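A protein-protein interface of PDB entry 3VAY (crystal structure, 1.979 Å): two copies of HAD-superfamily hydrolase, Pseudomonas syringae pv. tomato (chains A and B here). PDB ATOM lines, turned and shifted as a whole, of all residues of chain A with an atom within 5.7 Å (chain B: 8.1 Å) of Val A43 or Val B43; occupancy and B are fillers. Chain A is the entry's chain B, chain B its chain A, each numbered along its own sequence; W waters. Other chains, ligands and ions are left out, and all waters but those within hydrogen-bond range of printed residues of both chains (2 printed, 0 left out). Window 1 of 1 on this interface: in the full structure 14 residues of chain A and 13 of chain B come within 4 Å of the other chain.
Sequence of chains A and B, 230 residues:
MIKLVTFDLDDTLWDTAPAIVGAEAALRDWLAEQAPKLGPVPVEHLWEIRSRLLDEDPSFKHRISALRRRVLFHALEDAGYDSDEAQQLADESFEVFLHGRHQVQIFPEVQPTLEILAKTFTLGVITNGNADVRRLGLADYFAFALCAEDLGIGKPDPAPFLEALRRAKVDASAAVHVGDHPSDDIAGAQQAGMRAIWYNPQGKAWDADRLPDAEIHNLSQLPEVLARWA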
ATOM      1  N   GLU A  24      -7.273 -20.499 -31.343  1.00  0.00           N
ATOM      2  CA  GLU A  24      -6.714 -20.300 -30.015  1.00  0.00           C
ATOM      3  C   GLU A  24      -6.530 -18.810 -29.746  1.00  0.00           C
ATOM      4  O   GLU A  24      -6.925 -18.309 -28.692  1.00  0.00           O
ATOM      5  CB  GLU A  24      -5.384 -21.058 -29.862  1.00  0.00           C
ATOM      6  CG  GLU A  24      -5.563 -22.564 -29.686  1.00  0.00           C
ATOM      7  CD  GLU A  24      -4.254 -23.344 -29.721  1.00  0.00           C
ATOM      8  OE1 GLU A  24      -3.193 -22.738 -29.975  1.00  0.00           O
ATOM      9  OE2 GLU A  24      -4.294 -24.573 -29.491  1.00  0.00           O
ATOM     10  N   VAL A  41      -3.226 -16.377 -19.190  1.00  0.00           N
ATOM     11  CA  VAL A  41      -3.258 -17.737 -18.671  1.00  0.00           C
ATOM     12  C   VAL A  41      -2.236 -18.636 -19.360  1.00  0.00           C
ATOM     13  O   VAL A  41      -2.271 -18.819 -20.575  1.00  0.00           O
ATOM     14  CB  VAL A  41      -4.652 -18.344 -18.885  1.00  0.00           C
ATOM     15  CG1 VAL A  41      -5.138 -18.056 -20.309  1.00  0.00           C
ATOM     16  CG2 VAL A  41      -4.636 -19.829 -18.598  1.00  0.00           C
ATOM     17  N   PRO A  42      -1.323 -19.210 -18.582  1.00  0.00           N
ATOM     18  CA  PRO A  42      -0.333 -20.094 -19.199  1.00  0.00           C
ATOM     19  C   PRO A  42      -0.969 -21.385 -19.699  1.00  0.00           C
ATOM     20  O   PRO A  42      -1.775 -22.002 -18.990  1.00  0.00           O
ATOM     21  CB  PRO A  42       0.640 -20.384 -18.056  1.00  0.00           C
ATOM     22  CG  PRO A  42      -0.144 -20.142 -16.814  1.00  0.00           C
ATOM     23  CD  PRO A  42      -1.117 -19.057 -17.133  1.00  0.00           C
ATOM     24  N   VAL A  43      -0.618 -21.763 -20.927  1.00  0.00           N
ATOM     25  CA  VAL A  43      -0.998 -23.051 -21.499  1.00  0.00           C
ATOM     26  C   VAL A  43      -0.979 -24.120 -20.417  1.00  0.00           C
ATOM     27  O   VAL A  43      -1.871 -24.969 -20.327  1.00  0.00           O
ATOM     28  CB  VAL A  43      -0.010 -23.455 -22.612  1.00  0.00           C
ATOM     29  CG1 VAL A  43      -0.208 -24.907 -23.007  1.00  0.00           C
ATOM     30  CG2 VAL A  43      -0.160 -22.537 -23.797  1.00  0.00           C
ATOM     31  N   GLU A  44       0.035 -24.043 -19.571  1.00  0.00           N
ATOM     32  CA  GLU A  44       0.219 -25.006 -18.504  1.00  0.00           C
ATOM     33  C   GLU A  44      -1.010 -25.166 -17.611  1.00  0.00           C
ATOM     34  O   GLU A  44      -1.287 -26.259 -17.126  1.00  0.00           O
ATOM     35  CB  GLU A  44       1.440 -24.619 -17.664  1.00  0.00           C
ATOM     36  CG  GLU A  44       1.918 -25.734 -16.758  1.00  0.00           C
ATOM     37  CD  GLU A  44       2.274 -26.992 -17.531  1.00  0.00           C
ATOM     38  OE1 GLU A  44       2.758 -26.876 -18.680  1.00  0.00           O
ATOM     39  OE2 GLU A  44       2.063 -28.100 -16.990  1.00  0.00           O
ATOM     40  N   HIS A  45      -1.739 -24.071 -17.407  1.00  0.00           N
ATOM     41  CA  HIS A  45      -2.853 -24.016 -16.464  1.00  0.00           C
ATOM     42  C   HIS A  45      -4.135 -24.711 -16.937  1.00  0.00           C
ATOM     43  O   HIS A  45      -4.827 -25.358 -16.152  1.00  0.00           O
ATOM     44  CB  HIS A  45      -3.154 -22.562 -16.099  1.00  0.00           C
ATOM     45  N   LEU A  46      -4.475 -24.542 -18.208  1.00  0.00           N
ATOM     46  CA  LEU A  46      -5.655 -25.197 -18.766  1.00  0.00           C
ATOM     47  C   LEU A  46      -5.439 -26.693 -18.699  1.00  0.00           C
ATOM     48  O   LEU A  46      -6.366 -27.467 -18.462  1.00  0.00           O
ATOM     49  CB  LEU A  46      -5.846 -24.803 -20.228  1.00  0.00           C
ATOM     50  CG  LEU A  46      -5.958 -23.309 -20.484  1.00  0.00           C
ATOM     51  CD1 LEU A  46      -7.023 -22.756 -19.568  1.00  0.00           C
ATOM     52  CD2 LEU A  46      -4.603 -22.639 -20.260  1.00  0.00           C
ATOM     53  N   TRP A  47      -4.193 -27.081 -18.917  1.00  0.00           N
ATOM     54  CA  TRP A  47      -3.815 -28.480 -18.940  1.00  0.00           C
ATOM     55  C   TRP A  47      -3.957 -29.158 -17.591  1.00  0.00           C
ATOM     56  O   TRP A  47      -4.444 -30.290 -17.510  1.00  0.00           O
ATOM     57  CB  TRP A  47      -2.392 -28.594 -19.429  1.00  0.00           C
ATOM     58  CG  TRP A  47      -2.304 -28.384 -20.878  1.00  0.00           C
ATOM     59  CD1 TRP A  47      -3.335 -28.108 -21.746  1.00  0.00           C
ATOM     60  CD2 TRP A  47      -1.124 -28.442 -21.663  1.00  0.00           C
ATOM     61  NE1 TRP A  47      -2.849 -27.986 -23.026  1.00  0.00           N
ATOM     62  CE2 TRP A  47      -1.495 -28.194 -23.001  1.00  0.00           C
ATOM     63  CE3 TRP A  47       0.219 -28.682 -21.366  1.00  0.00           C
ATOM     64  CZ2 TRP A  47      -0.578 -28.183 -24.029  1.00  0.00           C
ATOM     65  CZ3 TRP A  47       1.123 -28.662 -22.386  1.00  0.00           C
ATOM     66  CH2 TRP A  47       0.724 -28.417 -23.707  1.00  0.00           C
ATOM     67  N   GLU A  48      -3.507 -28.477 -16.544  1.00  0.00           N
ATOM     68  CA  GLU A  48      -3.745 -28.935 -15.180  1.00  0.00           C
ATOM     69  C   GLU A  48      -5.222 -29.257 -14.991  1.00  0.00           C
ATOM     70  O   GLU A  48      -5.569 -30.302 -14.460  1.00  0.00           O
ATOM     71  CB  GLU A  48      -3.308 -27.871 -14.165  1.00  0.00           C
ATOM     72  CG  GLU A  48      -1.799 -27.750 -13.972  1.00  0.00           C
ATOM     73  CD  GLU A  48      -1.184 -28.965 -13.283  1.00  0.00           C
ATOM     74  OE1 GLU A  48      -1.948 -29.849 -12.826  1.00  0.00           O
ATOM     75  OE2 GLU A  48       0.066 -29.039 -13.200  1.00  0.00           O
ATOM     76  N   ALA B  17       1.458 -17.092 -12.556  1.00  0.00           N
ATOM     77  CA  ALA B  17       1.122 -16.869 -13.973  1.00  0.00           C
ATOM     78  C   ALA B  17       2.090 -16.035 -14.833  1.00  0.00           C
ATOM     79  O   ALA B  17       2.457 -16.473 -15.918  1.00  0.00           O
ATOM     80  CB  ALA B  17      -0.322 -16.342 -14.119  1.00  0.00           C
ATOM     81  N   ILE B  20       5.571 -17.486 -16.164  1.00  0.00           N
ATOM     82  CA  ILE B  20       5.399 -18.655 -17.013  1.00  0.00           C
ATOM     83  C   ILE B  20       4.845 -18.249 -18.379  1.00  0.00           C
ATOM     84  O   ILE B  20       5.257 -18.783 -19.409  1.00  0.00           O
ATOM     85  CB  ILE B  20       4.494 -19.707 -16.356  1.00  0.00           C
ATOM     86  CG1 ILE B  20       5.205 -20.332 -15.153  1.00  0.00           C
ATOM     87  CG2 ILE B  20       4.087 -20.792 -17.366  1.00  0.00           C
ATOM     88  CD1 ILE B  20       4.344 -21.298 -14.362  1.00  0.00           C
ATOM     89  N   VAL B  21       3.917 -17.299 -18.387  1.00  0.00           N
ATOM     90  CA  VAL B  21       3.427 -16.734 -19.639  1.00  0.00           C
ATOM     91  C   VAL B  21       4.572 -16.138 -20.446  1.00  0.00           C
ATOM     92  O   VAL B  21       4.714 -16.414 -21.637  1.00  0.00           O
ATOM     93  CB  VAL B  21       2.357 -15.655 -19.388  1.00  0.00           C
ATOM     94  CG1 VAL B  21       2.191 -14.762 -20.610  1.00  0.00           C
ATOM     95  CG2 VAL B  21       1.034 -16.312 -19.004  1.00  0.00           C
ATOM     96  N   GLU B  24       6.698 -18.949 -21.873  1.00  0.00           N
ATOM     97  CA  GLU B  24       6.089 -19.577 -23.030  1.00  0.00           C
ATOM     98  C   GLU B  24       6.309 -18.714 -24.274  1.00  0.00           C
ATOM     99  O   GLU B  24       6.640 -19.228 -25.340  1.00  0.00           O
ATOM    100  CB  GLU B  24       4.599 -19.850 -22.786  1.00  0.00           C
ATOM    101  CG  GLU B  24       4.334 -21.082 -21.906  1.00  0.00           C
ATOM    102  CD  GLU B  24       2.873 -21.222 -21.468  1.00  0.00           C
ATOM    103  OE1 GLU B  24       2.063 -20.305 -21.733  1.00  0.00           O
ATOM    104  OE2 GLU B  24       2.538 -22.256 -20.851  1.00  0.00           O
ATOM    105  N   PRO B  40       4.327 -22.249 -36.466  1.00  0.00           N
ATOM    106  CA  PRO B  40       3.272 -22.023 -35.471  1.00  0.00           C
ATOM    107  C   PRO B  40       2.558 -23.320 -35.105  1.00  0.00           C
ATOM    108  O   PRO B  40       1.801 -23.881 -35.905  1.00  0.00           O
ATOM    109  CB  PRO B  40       2.313 -21.068 -36.186  1.00  0.00           C
ATOM    110  CG  PRO B  40       3.167 -20.359 -37.188  1.00  0.00           C
ATOM    111  CD  PRO B  40       4.179 -21.373 -37.643  1.00  0.00           C
ATOM    112  N   VAL B  41       2.810 -23.791 -33.891  1.00  0.00           N
ATOM    113  CA  VAL B  41       2.229 -25.043 -33.434  1.00  0.00           C
ATOM    114  C   VAL B  41       1.144 -24.810 -32.385  1.00  0.00           C
ATOM    115  O   VAL B  41       1.389 -24.185 -31.349  1.00  0.00           O
ATOM    116  CB  VAL B  41       3.317 -26.005 -32.902  1.00  0.00           C
ATOM    117  CG1 VAL B  41       4.651 -25.285 -32.762  1.00  0.00           C
ATOM    118  CG2 VAL B  41       2.889 -26.644 -31.586  1.00  0.00           C
ATOM    119  N   PRO B  42      -0.065 -25.303 -32.665  1.00  0.00           N
ATOM    120  CA  PRO B  42      -1.179 -25.195 -31.724  1.00  0.00           C
ATOM    121  C   PRO B  42      -0.886 -25.881 -30.393  1.00  0.00           C
ATOM    122  O   PRO B  42      -0.334 -26.985 -30.352  1.00  0.00           O
ATOM    123  CB  PRO B  42      -2.337 -25.889 -32.455  1.00  0.00           C
ATOM    124  CG  PRO B  42      -1.711 -26.634 -33.594  1.00  0.00           C
ATOM    125  CD  PRO B  42      -0.477 -25.882 -33.953  1.00  0.00           C
ATOM    126  N   VAL B  43      -1.238 -25.194 -29.312  1.00  0.00           N
ATOM    127  CA  VAL B  43      -1.150 -25.737 -27.964  1.00  0.00           C
ATOM    128  C   VAL B  43      -1.689 -27.159 -27.952  1.00  0.00           C
ATOM    129  O   VAL B  43      -1.196 -28.045 -27.239  1.00  0.00           O
ATOM    130  CB  VAL B  43      -2.007 -24.897 -26.996  1.00  0.00           C
ATOM    131  CG1 VAL B  43      -2.147 -25.595 -25.654  1.00  0.00           C
ATOM    132  CG2 VAL B  43      -1.428 -23.504 -26.849  1.00  0.00           C
ATOM    133  N   GLU B  44      -2.684 -27.390 -28.754  1.00  0.00           N
ATOM    134  CA  GLU B  44      -3.309 -28.687 -28.832  1.00  0.00           C
ATOM    135  C   GLU B  44      -2.362 -29.782 -29.306  1.00  0.00           C
ATOM    136  O   GLU B  44      -2.461 -30.890 -28.902  1.00  0.00           O
ATOM    137  CB  GLU B  44      -4.587 -28.585 -29.671  1.00  0.00           C
ATOM    138  CG  GLU B  44      -5.526 -29.734 -29.557  1.00  0.00           C
ATOM    139  CD  GLU B  44      -6.077 -29.939 -28.200  1.00  0.00           C
ATOM    140  OE1 GLU B  44      -6.136 -28.981 -27.438  1.00  0.00           O
ATOM    141  OE2 GLU B  44      -6.453 -31.071 -27.881  1.00  0.00           O
ATOM    142  N   HIS B  45      -1.423 -29.416 -30.149  1.00  0.00           N
ATOM    143  CA  HIS B  45      -0.477 -30.315 -30.743  1.00  0.00           C
ATOM    144  C   HIS B  45       0.630 -30.725 -29.781  1.00  0.00           C
ATOM    145  O   HIS B  45       1.160 -31.797 -29.871  1.00  0.00           O
ATOM    146  CB  HIS B  45       0.090 -29.714 -32.038  1.00  0.00           C
ATOM    147  CG  HIS B  45      -0.853 -29.765 -33.209  1.00  0.00           C
ATOM    148  ND1 HIS B  45      -2.211 -29.957 -33.078  1.00  0.00           N
ATOM    149  CD2 HIS B  45      -0.623 -29.670 -34.540  1.00  0.00           C
ATOM    150  CE1 HIS B  45      -2.773 -29.950 -34.267  1.00  0.00           C
ATOM    151  NE2 HIS B  45      -1.829 -29.790 -35.172  1.00  0.00           N
ATOM    152  N   LEU B  46       0.950 -29.873 -28.829  1.00  0.00           N
ATOM    153  CA  LEU B  46       1.932 -30.262 -27.825  1.00  0.00           C
ATOM    154  C   LEU B  46       1.287 -31.209 -26.817  1.00  0.00           C
ATOM    155  O   LEU B  46       1.929 -32.128 -26.305  1.00  0.00           O
ATOM    156  CB  LEU B  46       2.493 -29.022 -27.131  1.00  0.00           C
ATOM    157  CG  LEU B  46       3.107 -28.078 -28.163  1.00  0.00           C
ATOM    158  CD1 LEU B  46       3.110 -26.637 -27.672  1.00  0.00           C
ATOM    159  CD2 LEU B  46       4.494 -28.566 -28.538  1.00  0.00           C
ATOM    160  N   TRP B  47       0.019 -30.983 -26.531  1.00  0.00           N
ATOM    161  CA  TRP B  47      -0.731 -31.777 -25.569  1.00  0.00           C
ATOM    162  C   TRP B  47      -0.798 -33.226 -26.028  1.00  0.00           C
ATOM    163  O   TRP B  47      -0.630 -34.131 -25.248  1.00  0.00           O
ATOM    164  CB  TRP B  47      -2.109 -31.166 -25.264  1.00  0.00           C
ATOM    165  CG  TRP B  47      -3.208 -32.117 -24.688  1.00  0.00           C
ATOM    166  CD1 TRP B  47      -4.037 -32.934 -25.396  1.00  0.00           C
ATOM    167  CD2 TRP B  47      -3.566 -32.311 -23.309  1.00  0.00           C
ATOM    168  NE1 TRP B  47      -4.861 -33.608 -24.569  1.00  0.00           N
ATOM    169  CE2 TRP B  47      -4.608 -33.243 -23.280  1.00  0.00           C
ATOM    170  CE3 TRP B  47      -3.105 -31.786 -22.109  1.00  0.00           C
ATOM    171  CZ2 TRP B  47      -5.183 -33.678 -22.111  1.00  0.00           C
ATOM    172  CZ3 TRP B  47      -3.691 -32.214 -20.942  1.00  0.00           C
ATOM    173  CH2 TRP B  47      -4.707 -33.157 -20.945  1.00  0.00           C
ATOM    174  N   GLU B  48      -0.986 -33.446 -27.316  1.00  0.00           N
ATOM    175  CA  GLU B  48      -1.017 -34.809 -27.832  1.00  0.00           C
ATOM    176  C   GLU B  48       0.283 -35.553 -27.643  1.00  0.00           C
ATOM    177  O   GLU B  48       0.284 -36.681 -27.312  1.00  0.00           O
ATOM    178  CB  GLU B  48      -1.472 -34.835 -29.277  1.00  0.00           C
ATOM    179  CG  GLU B  48      -2.842 -34.230 -29.496  1.00  0.00           C
ATOM    180  CD  GLU B  48      -3.993 -35.237 -29.471  1.00  0.00           C
ATOM    181  OE1 GLU B  48      -5.163 -34.842 -29.692  1.00  0.00           O
ATOM    182  OE2 GLU B  48      -3.720 -36.416 -29.215  1.00  0.00           O
ATOM    183  N   ILE B  49       1.393 -34.885 -27.849  1.00  0.00           N
ATOM    184  CA  ILE B  49       2.710 -35.484 -27.662  1.00  0.00           C
ATOM    185  C   ILE B  49       2.953 -35.715 -26.178  1.00  0.00           C
ATOM    186  O   ILE B  49       3.410 -36.781 -25.756  1.00  0.00           O
ATOM    187  CB  ILE B  49       3.820 -34.581 -28.211  1.00  0.00           C
ATOM    188  CG1 ILE B  49       3.622 -34.361 -29.709  1.00  0.00           C
ATOM    189  CG2 ILE B  49       5.190 -35.191 -27.924  1.00  0.00           C
ATOM    190  CD1 ILE B  49       4.403 -33.188 -30.256  1.00  0.00           C
ATOM    191  N   ARG B  50       2.644 -34.694 -25.390  1.00  0.00           N
ATOM    192  CA  ARG B  50       2.738 -34.793 -23.945  1.00  0.00           C
ATOM    193  C   ARG B  50       1.931 -35.990 -23.442  1.00  0.00           C
ATOM    194  O   ARG B  50       2.421 -36.784 -22.641  1.00  0.00           O
ATOM    195  CB  ARG B  50       2.225 -33.505 -23.299  1.00  0.00           C
ATOM    196  CG  ARG B  50       2.544 -33.387 -21.829  1.00  0.00           C
ATOM    197  CD  ARG B  50       1.909 -32.145 -21.212  1.00  0.00           C
ATOM    198  NE  ARG B  50       2.337 -31.990 -19.823  1.00  0.00           N
ATOM    199  CZ  ARG B  50       2.945 -30.911 -19.343  1.00  0.00           C
ATOM    200  NH1 ARG B  50       3.173 -29.868 -20.132  1.00  0.00           N
ATOM    201  NH2 ARG B  50       3.304 -30.862 -18.070  1.00  0.00           N
ATOM    202  N   ARG B  68       9.102 -31.630 -20.817  1.00  0.00           N
ATOM    203  CA  ARG B  68       9.000 -30.576 -21.822  1.00  0.00           C
ATOM    204  C   ARG B  68      10.112 -30.691 -22.874  1.00  0.00           C
ATOM    205  O   ARG B  68       9.879 -30.467 -24.060  1.00  0.00           O
ATOM    206  CB  ARG B  68       9.007 -29.187 -21.181  1.00  0.00           C
ATOM    207  CG  ARG B  68       8.736 -28.052 -22.173  1.00  0.00           C
ATOM    208  CD  ARG B  68       8.549 -26.707 -21.460  1.00  0.00           C
ATOM    209  NE  ARG B  68       7.346 -26.696 -20.625  1.00  0.00           N
ATOM    210  CZ  ARG B  68       6.181 -26.169 -20.989  1.00  0.00           C
ATOM    211  NH1 ARG B  68       6.053 -25.593 -22.173  1.00  0.00           N
ATOM    212  NH2 ARG B  68       5.143 -26.214 -20.168  1.00  0.00           N
ATOM    213  N   VAL B  71       9.082 -33.383 -25.267  1.00  0.00           N
ATOM    214  CA  VAL B  71       8.006 -32.914 -26.132  1.00  0.00           C
ATOM    215  C   VAL B  71       8.544 -31.992 -27.220  1.00  0.00           C
ATOM    216  O   VAL B  71       8.148 -32.086 -28.378  1.00  0.00           O
ATOM    217  CB  VAL B  71       6.907 -32.161 -25.336  1.00  0.00           C
ATOM    218  CG1 VAL B  71       5.943 -31.463 -26.287  1.00  0.00           C
ATOM    219  CG2 VAL B  71       6.165 -33.117 -24.403  1.00  0.00           C
HETATM  220  O   HOH W   1      -5.392 -25.739 -27.003  1.00  0.00           O
HETATM  221  O   HOH W   2      -4.733 -28.052 -24.859  1.00  0.00           O
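Glu A24 touches Pro B42, and with the chains exchanged Pro A42 touches Glu B24.
Glu A24 touches Val B43, and with the chains exchanged Val A43 touches Glu B24.
Glu A24 touches Glu B44, and with the chains exchanged Glu A44 touches Glu B24.
Val B43 touches its own counterpart, Val A43.
Positions printed for both chains: 24, 41, 42, 43, 44, 45, 46, 47 and 48.
Of the 15 pairs that touch across the chains among the printed residues, 8 have their exchanged pair printed and touching as well.
Val A43 touches two residues of chain B.
Val B43 touches just these residues of chain A: Glu A24, Val A43 and Trp A47.
Of the printed residues of chain A, Ile B20 touches Pro A42 (3.5 Å).
Printed residues of chain A within 4 Å of Trp B47: Trp A47.
Of the printed residues of chain A, Glu B44 touches Glu A24.
Printed residues of chain A within 4 Å of Val B21: Pro A42.
His B45 touches none of the printed residues of chain A.
The nearest printed residue of chain B that does not touch Val A43 is Ile B20 (6.0 Å).
The nearest printed residue of chain A that does not touch Val B43 is Leu A46 (6.6 Å).
Among the printed residues, merely in contact across the chains: Trp A47 with Val B43 (3.3 Å), Trp A47 with Arg B50 (3.3 Å), Val A43 with Val B43 (3.4 Å), Pro A42 with Glu B24 (3.5 Å), Pro A42 with Ile B20 (3.5 Å), Trp A47 with Trp B47 (3.6 Å), Glu A24 with Pro B42 (3.6 Å), Pro A42 with Val B21 (3.8 Å) and Trp A47 with Leu B46 (3.9 Å).
The side-chain carboxylate (OE1) of Glu B24 lies within hydrogen-bond range of the backbone NH (N) of Val A43.
The backbone NH (N) of Glu A44 sits at hydrogen-bond distance from the side-chain carboxylate (OE2) of Glu B24, at 3.3 Å.
The backbone NH (N) of Val B43 lies within hydrogen-bond range of the side-chain carboxylate (OE2) of Glu A24.
The backbone NH (N) of Glu B44 is in hydrogen-bond range of the side-chain carboxylate (OE2) of Glu A24 (3.3 Å).
The side-chain carboxylate (OE2) of Glu A44 is in salt-bridge range of the guanidinium group (NH2) of Arg B50, at 3.2 Å.
OE1 of Glu A44 lies within salt-bridge range of NH2 of Arg B68 (2.9 Å).
Water W2 lies within hydrogen-bond range of NE1 of Trp A47 and OE1 of Glu B44.
Water W1 bridges OE2 of Glu A24 (3.0 Å) and OE1 of Glu B44 (3.4 Å).
Of the 17 printed residues of chain B, 10 touch a printed residue of chain A.
Hydrophobic or aromatic side chains of chain A that line the printed part of chain B: Pro A42, Val A43 and Trp A47.
Along chain A the printed residues that touch a printed residue of chain B span positions 24 to 47.
Among the printed residues, Asp or Glu carboxylates within 4 Å of a Lys or Arg side-chain nitrogen of the other chain: Glu A44 with Arg B50 and Glu A44 with Arg B68.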
